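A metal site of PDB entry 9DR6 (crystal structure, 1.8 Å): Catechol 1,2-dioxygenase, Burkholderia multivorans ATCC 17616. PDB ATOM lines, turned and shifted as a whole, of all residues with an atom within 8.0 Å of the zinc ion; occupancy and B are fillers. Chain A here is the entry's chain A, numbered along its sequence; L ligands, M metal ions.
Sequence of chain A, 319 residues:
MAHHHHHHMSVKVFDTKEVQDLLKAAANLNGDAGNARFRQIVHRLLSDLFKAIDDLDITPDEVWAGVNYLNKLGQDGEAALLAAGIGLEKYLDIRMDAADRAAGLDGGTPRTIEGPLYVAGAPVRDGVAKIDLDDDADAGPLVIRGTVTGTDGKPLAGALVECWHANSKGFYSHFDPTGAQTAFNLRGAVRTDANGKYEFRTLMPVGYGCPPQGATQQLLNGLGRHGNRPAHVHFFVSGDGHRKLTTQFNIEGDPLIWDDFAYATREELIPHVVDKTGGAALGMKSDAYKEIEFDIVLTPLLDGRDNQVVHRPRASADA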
ATOM      1  N   ILE A 113       8.514 -10.514  -0.659  1.00  0.00           N
ATOM      2  CA  ILE A 113       9.170 -11.598  -1.371  1.00  0.00           C
ATOM      3  C   ILE A 113      10.393 -11.094  -2.127  1.00  0.00           C
ATOM      4  O   ILE A 113      10.416  -9.973  -2.660  1.00  0.00           O
ATOM      5  CB  ILE A 113       8.191 -12.332  -2.304  1.00  0.00           C
ATOM      6  CG1 ILE A 113       7.788 -11.460  -3.491  1.00  0.00           C
ATOM      7  CG2 ILE A 113       6.979 -12.841  -1.514  1.00  0.00           C
ATOM      8  CD1 ILE A 113       6.960 -12.209  -4.517  1.00  0.00           C
ATOM      9  N   GLU A 114      11.418 -11.949  -2.187  1.00  0.00           N
ATOM     10  CA  GLU A 114      12.601 -11.643  -2.979  1.00  0.00           C
ATOM     11  C   GLU A 114      12.317 -11.663  -4.479  1.00  0.00           C
ATOM     12  O   GLU A 114      12.825 -10.811  -5.217  1.00  0.00           O
ATOM     13  CB  GLU A 114      13.706 -12.657  -2.636  1.00  0.00           C
ATOM     14  CG  GLU A 114      14.994 -12.460  -3.390  1.00  0.00           C
ATOM     15  CD  GLU A 114      16.057 -13.461  -2.968  1.00  0.00           C
ATOM     16  OE1 GLU A 114      16.000 -13.918  -1.805  1.00  0.00           O
ATOM     17  OE2 GLU A 114      16.934 -13.809  -3.814  1.00  0.00           O
ATOM     18  N   GLY A 115      11.507 -12.603  -4.939  1.00  0.00           N
ATOM     19  CA  GLY A 115      11.352 -12.831  -6.364  1.00  0.00           C
ATOM     20  C   GLY A 115      12.576 -13.556  -6.901  1.00  0.00           C
ATOM     21  O   GLY A 115      13.556 -13.763  -6.177  1.00  0.00           O
ATOM     22  N   PRO A 116      12.551 -13.930  -8.176  1.00  0.00           N
ATOM     23  CA  PRO A 116      13.601 -14.822  -8.691  1.00  0.00           C
ATOM     24  C   PRO A 116      14.715 -14.147  -9.474  1.00  0.00           C
ATOM     25  O   PRO A 116      15.503 -14.832 -10.143  1.00  0.00           O
ATOM     26  CB  PRO A 116      12.797 -15.775  -9.592  1.00  0.00           C
ATOM     27  CG  PRO A 116      11.706 -14.894 -10.159  1.00  0.00           C
ATOM     28  CD  PRO A 116      11.356 -13.889  -9.055  1.00  0.00           C
ATOM     29  N   LEU A 117      14.859 -12.829  -9.356  1.00  0.00           N
ATOM     30  CA  LEU A 117      15.691 -12.079 -10.298  1.00  0.00           C
ATOM     31  C   LEU A 117      16.861 -11.335  -9.641  1.00  0.00           C
ATOM     32  O   LEU A 117      17.417 -10.423 -10.257  1.00  0.00           O
ATOM     33  CB  LEU A 117      14.815 -11.106 -11.082  1.00  0.00           C
ATOM     34  CG  LEU A 117      13.668 -11.763 -11.848  1.00  0.00           C
ATOM     35  CD1 LEU A 117      12.926 -10.719 -12.637  1.00  0.00           C
ATOM     36  CD2 LEU A 117      14.186 -12.859 -12.766  1.00  0.00           C
ATOM     37  N   TYR A 118      17.261 -11.708  -8.434  1.00  0.00           N
ATOM     38  CA  TYR A 118      18.465 -11.138  -7.856  1.00  0.00           C
ATOM     39  C   TYR A 118      19.700 -11.574  -8.636  1.00  0.00           C
ATOM     40  O   TYR A 118      19.775 -12.712  -9.108  1.00  0.00           O
ATOM     41  CB  TYR A 118      18.626 -11.562  -6.395  1.00  0.00           C
ATOM     42  CG  TYR A 118      19.846 -10.983  -5.710  1.00  0.00           C
ATOM     43  CD1 TYR A 118      19.936  -9.627  -5.406  1.00  0.00           C
ATOM     44  CD2 TYR A 118      20.914 -11.796  -5.359  1.00  0.00           C
ATOM     45  CE1 TYR A 118      21.055  -9.101  -4.780  1.00  0.00           C
ATOM     46  CE2 TYR A 118      22.029 -11.287  -4.733  1.00  0.00           C
ATOM     47  CZ  TYR A 118      22.091  -9.940  -4.429  1.00  0.00           C
ATOM     48  OH  TYR A 118      23.213  -9.463  -3.805  1.00  0.00           O
ATOM     49  N   TRP A 164      17.444  -3.672  -6.805  1.00  0.00           N
ATOM     50  CA  TRP A 164      17.396  -4.046  -8.215  1.00  0.00           C
ATOM     51  C   TRP A 164      15.976  -3.830  -8.703  1.00  0.00           C
ATOM     52  O   TRP A 164      15.020  -3.979  -7.927  1.00  0.00           O
ATOM     53  CB  TRP A 164      17.878  -5.497  -8.433  1.00  0.00           C
ATOM     54  CG  TRP A 164      17.105  -6.636  -7.784  1.00  0.00           C
ATOM     55  CD1 TRP A 164      16.261  -7.506  -8.397  1.00  0.00           C
ATOM     56  CD2 TRP A 164      17.149  -7.035  -6.399  1.00  0.00           C
ATOM     57  NE1 TRP A 164      15.775  -8.425  -7.499  1.00  0.00           N
ATOM     58  CE2 TRP A 164      16.292  -8.154  -6.266  1.00  0.00           C
ATOM     59  CE3 TRP A 164      17.827  -6.566  -5.264  1.00  0.00           C
ATOM     60  CZ2 TRP A 164      16.090  -8.795  -5.039  1.00  0.00           C
ATOM     61  CZ3 TRP A 164      17.619  -7.211  -4.044  1.00  0.00           C
ATOM     62  CH2 TRP A 164      16.757  -8.321  -3.939  1.00  0.00           C
ATOM     63  N   HIS A 165      15.841  -3.446  -9.968  1.00  0.00           N
ATOM     64  CA  HIS A 165      14.524  -3.196 -10.540  1.00  0.00           C
ATOM     65  C   HIS A 165      14.588  -3.231 -12.063  1.00  0.00           C
ATOM     66  O   HIS A 165      15.661  -3.291 -12.657  1.00  0.00           O
ATOM     67  CB  HIS A 165      13.938  -1.854 -10.029  1.00  0.00           C
ATOM     68  CG  HIS A 165      14.649  -0.631 -10.525  1.00  0.00           C
ATOM     69  ND1 HIS A 165      14.405  -0.078 -11.761  1.00  0.00           N
ATOM     70  CD2 HIS A 165      15.536   0.185  -9.914  1.00  0.00           C
ATOM     71  CE1 HIS A 165      15.142   1.009 -11.910  1.00  0.00           C
ATOM     72  NE2 HIS A 165      15.843   1.191 -10.808  1.00  0.00           N
ATOM     73  N   ALA A 166      13.400  -3.209 -12.673  1.00  0.00           N
ATOM     74  CA  ALA A 166      13.197  -3.333 -14.107  1.00  0.00           C
ATOM     75  C   ALA A 166      13.364  -2.011 -14.853  1.00  0.00           C
ATOM     76  O   ALA A 166      13.262  -0.923 -14.276  1.00  0.00           O
ATOM     77  CB  ALA A 166      11.784  -3.867 -14.393  1.00  0.00           C
ATOM     78  N   GLY A 170       9.983  -3.455 -18.686  1.00  0.00           N
ATOM     79  CA  GLY A 170       9.695  -4.487 -17.723  1.00  0.00           C
ATOM     80  C   GLY A 170      10.777  -5.513 -17.551  1.00  0.00           C
ATOM     81  O   GLY A 170      10.551  -6.521 -16.870  1.00  0.00           O
ATOM     82  N   TYR A 172      14.700  -6.910 -16.519  1.00  0.00           N
ATOM     83  CA  TYR A 172      15.844  -6.787 -15.627  1.00  0.00           C
ATOM     84  C   TYR A 172      17.128  -7.173 -16.348  1.00  0.00           C
ATOM     85  O   TYR A 172      17.132  -8.096 -17.165  1.00  0.00           O
ATOM     86  CB  TYR A 172      15.695  -7.718 -14.426  1.00  0.00           C
ATOM     87  CG  TYR A 172      14.616  -7.372 -13.438  1.00  0.00           C
ATOM     88  CD1 TYR A 172      13.280  -7.573 -13.725  1.00  0.00           C
ATOM     89  CD2 TYR A 172      14.944  -6.855 -12.201  1.00  0.00           C
ATOM     90  CE1 TYR A 172      12.290  -7.255 -12.816  1.00  0.00           C
ATOM     91  CE2 TYR A 172      13.972  -6.548 -11.286  1.00  0.00           C
ATOM     92  CZ  TYR A 172      12.648  -6.752 -11.593  1.00  0.00           C
ATOM     93  OH  TYR A 172      11.669  -6.436 -10.706  1.00  0.00           O
ATOM     94  N   VAL A 206       8.992   0.124 -14.592  1.00  0.00           N
ATOM     95  CA  VAL A 206       7.634  -0.274 -14.915  1.00  0.00           C
ATOM     96  C   VAL A 206       7.470  -1.734 -14.493  1.00  0.00           C
ATOM     97  O   VAL A 206       8.451  -2.445 -14.258  1.00  0.00           O
ATOM     98  CB  VAL A 206       7.273  -0.086 -16.406  1.00  0.00           C
ATOM     99  CG1 VAL A 206       7.744   1.277 -16.896  1.00  0.00           C
ATOM    100  CG2 VAL A 206       7.845  -1.207 -17.254  1.00  0.00           C
ATOM    101  N   GLY A 207       6.218  -2.167 -14.422  1.00  0.00           N
ATOM    102  CA  GLY A 207       5.936  -3.483 -13.895  1.00  0.00           C
ATOM    103  C   GLY A 207       6.449  -4.597 -14.786  1.00  0.00           C
ATOM    104  O   GLY A 207       6.600  -4.447 -15.997  1.00  0.00           O
ATOM    105  N   TYR A 208       6.705  -5.742 -14.162  1.00  0.00           N
ATOM    106  CA  TYR A 208       7.201  -6.944 -14.822  1.00  0.00           C
ATOM    107  C   TYR A 208       6.024  -7.836 -15.209  1.00  0.00           C
ATOM    108  O   TYR A 208       4.964  -7.804 -14.595  1.00  0.00           O
ATOM    109  CB  TYR A 208       8.156  -7.683 -13.873  1.00  0.00           C
ATOM    110  CG  TYR A 208       8.532  -9.097 -14.252  1.00  0.00           C
ATOM    111  CD1 TYR A 208       7.684 -10.163 -13.989  1.00  0.00           C
ATOM    112  CD2 TYR A 208       9.774  -9.368 -14.841  1.00  0.00           C
ATOM    113  CE1 TYR A 208       8.036 -11.458 -14.320  1.00  0.00           C
ATOM    114  CE2 TYR A 208      10.120 -10.667 -15.179  1.00  0.00           C
ATOM    115  CZ  TYR A 208       9.254 -11.710 -14.915  1.00  0.00           C
ATOM    116  OH  TYR A 208       9.587 -12.994 -15.239  1.00  0.00           O
ATOM    117  N   ARG A 229       2.968  -7.866 -12.644  1.00  0.00           N
ATOM    118  CA  ARG A 229       3.307  -7.238 -11.395  1.00  0.00           C
ATOM    119  C   ARG A 229       3.277  -5.727 -11.544  1.00  0.00           C
ATOM    120  O   ARG A 229       3.643  -5.206 -12.607  1.00  0.00           O
ATOM    121  CB  ARG A 229       4.699  -7.656 -10.908  1.00  0.00           C
ATOM    122  CG  ARG A 229       4.976  -9.151 -10.971  1.00  0.00           C
ATOM    123  CD  ARG A 229       6.161  -9.496 -10.077  1.00  0.00           C
ATOM    124  NE  ARG A 229       5.804  -9.306  -8.680  1.00  0.00           N
ATOM    125  CZ  ARG A 229       6.667  -9.299  -7.671  1.00  0.00           C
ATOM    126  NH1 ARG A 229       7.966  -9.452  -7.874  1.00  0.00           N
ATOM    127  NH2 ARG A 229       6.213  -9.141  -6.432  1.00  0.00           N
ATOM    128  N   PRO A 230       2.863  -4.989 -10.514  1.00  0.00           N
ATOM    129  CA  PRO A 230       2.975  -3.535 -10.560  1.00  0.00           C
ATOM    130  C   PRO A 230       4.431  -3.127 -10.442  1.00  0.00           C
ATOM    131  O   PRO A 230       5.284  -3.911 -10.025  1.00  0.00           O
ATOM    132  CB  PRO A 230       2.174  -3.079  -9.335  1.00  0.00           C
ATOM    133  CG  PRO A 230       2.332  -4.227  -8.371  1.00  0.00           C
ATOM    134  CD  PRO A 230       2.321  -5.469  -9.230  1.00  0.00           C
ATOM    135  N   ALA A 231       4.724  -1.874 -10.802  1.00  0.00           N
ATOM    136  CA  ALA A 231       6.099  -1.376 -10.701  1.00  0.00           C
ATOM    137  C   ALA A 231       6.573  -1.354  -9.251  1.00  0.00           C
ATOM    138  O   ALA A 231       5.844  -0.954  -8.340  1.00  0.00           O
ATOM    139  CB  ALA A 231       6.190   0.034 -11.287  1.00  0.00           C
ATOM    140  N   HIS A 232       7.825  -1.756  -9.053  1.00  0.00           N
ATOM    141  CA  HIS A 232       8.397  -1.907  -7.717  1.00  0.00           C
ATOM    142  C   HIS A 232       9.913  -1.929  -7.801  1.00  0.00           C
ATOM    143  O   HIS A 232      10.503  -2.126  -8.873  1.00  0.00           O
ATOM    144  CB  HIS A 232       7.893  -3.202  -7.061  1.00  0.00           C
ATOM    145  CG  HIS A 232       8.286  -4.419  -7.828  1.00  0.00           C
ATOM    146  ND1 HIS A 232       7.648  -4.803  -8.988  1.00  0.00           N
ATOM    147  CD2 HIS A 232       9.300  -5.293  -7.649  1.00  0.00           C
ATOM    148  CE1 HIS A 232       8.235  -5.876  -9.474  1.00  0.00           C
ATOM    149  NE2 HIS A 232       9.222  -6.209  -8.671  1.00  0.00           N
ATOM    150  N   VAL A 233      10.530  -1.768  -6.636  1.00  0.00           N
ATOM    151  CA  VAL A 233      11.985  -1.813  -6.453  1.00  0.00           C
ATOM    152  C   VAL A 233      12.276  -2.772  -5.312  1.00  0.00           C
ATOM    153  O   VAL A 233      11.725  -2.622  -4.214  1.00  0.00           O
ATOM    154  CB  VAL A 233      12.564  -0.424  -6.114  1.00  0.00           C
ATOM    155  CG1 VAL A 233      14.073  -0.503  -5.911  1.00  0.00           C
ATOM    156  CG2 VAL A 233      12.230   0.564  -7.211  1.00  0.00           C
ATOM    157  N   HIS A 234      13.157  -3.734  -5.574  1.00  0.00           N
ATOM    158  CA  HIS A 234      13.598  -4.682  -4.568  1.00  0.00           C
ATOM    159  C   HIS A 234      14.735  -4.152  -3.722  1.00  0.00           C
ATOM    160  O   HIS A 234      15.610  -3.439  -4.220  1.00  0.00           O
ATOM    161  CB  HIS A 234      14.144  -5.949  -5.189  1.00  0.00           C
ATOM    162  CG  HIS A 234      13.153  -6.684  -6.002  1.00  0.00           C
ATOM    163  ND1 HIS A 234      12.371  -7.672  -5.459  1.00  0.00           N
ATOM    164  CD2 HIS A 234      12.798  -6.566  -7.290  1.00  0.00           C
ATOM    165  CE1 HIS A 234      11.578  -8.152  -6.404  1.00  0.00           C
ATOM    166  NE2 HIS A 234      11.831  -7.501  -7.510  1.00  0.00           N
ATOM    167  N   GLN A 248      10.761  -4.557  -0.391  1.00  0.00           N
ATOM    168  CA  GLN A 248      10.593  -3.828  -1.634  1.00  0.00           C
ATOM    169  C   GLN A 248       9.727  -2.624  -1.340  1.00  0.00           C
ATOM    170  O   GLN A 248       9.131  -2.510  -0.257  1.00  0.00           O
ATOM    171  CB  GLN A 248       9.946  -4.698  -2.715  1.00  0.00           C
ATOM    172  CG  GLN A 248       8.437  -4.708  -2.660  1.00  0.00           C
ATOM    173  CD  GLN A 248       7.825  -5.602  -3.714  1.00  0.00           C
ATOM    174  OE1 GLN A 248       8.507  -6.440  -4.311  1.00  0.00           O
ATOM    175  NE2 GLN A 248       6.536  -5.422  -3.964  1.00  0.00           N
HETATM  176 CL1  LIG L   1      10.709  -9.791  -9.519  1.00  0.00          CL
HETATM  177 ZN    ZN M   1      10.814  -7.554  -9.412  1.00  0.00          ZN
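The backbone NH of His 234 lies within hydrogen-bond range of the backbone carbonyl oxygen of Trp 164 (3.0 Å).
O of Glu 114 lies close to ND1 of His 234.
A ring nitrogen (ND1) of His 232 sits at hydrogen-bond distance from the backbone carbonyl oxygen (O) of Pro 230, at 2.7 Å.
The backbone NH (N) of Arg 229 lies within hydrogen-bond range of the backbone carbonyl oxygen (O) of Tyr 208, at 2.8 Å.
Merely in contact with the zinc ion: Arg 229 (3.8 Å).
Four residues have an atom within 4 Å of the zinc ion: Tyr 172, Arg 229, His 232 and His 234.
The nearest printed residue that does not touch the zinc ion is Leu 117 (5.0 Å).
The zinc ion is bound by the side-chain hydroxyl (OH) of Tyr 172 (1.9 Å), a ring nitrogen (NE2) of His 234 (2.2 Å), a ring nitrogen (NE2) of His 232 (2.2 Å) and a chlorine (CL1) of the ligand (2.2 Å).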
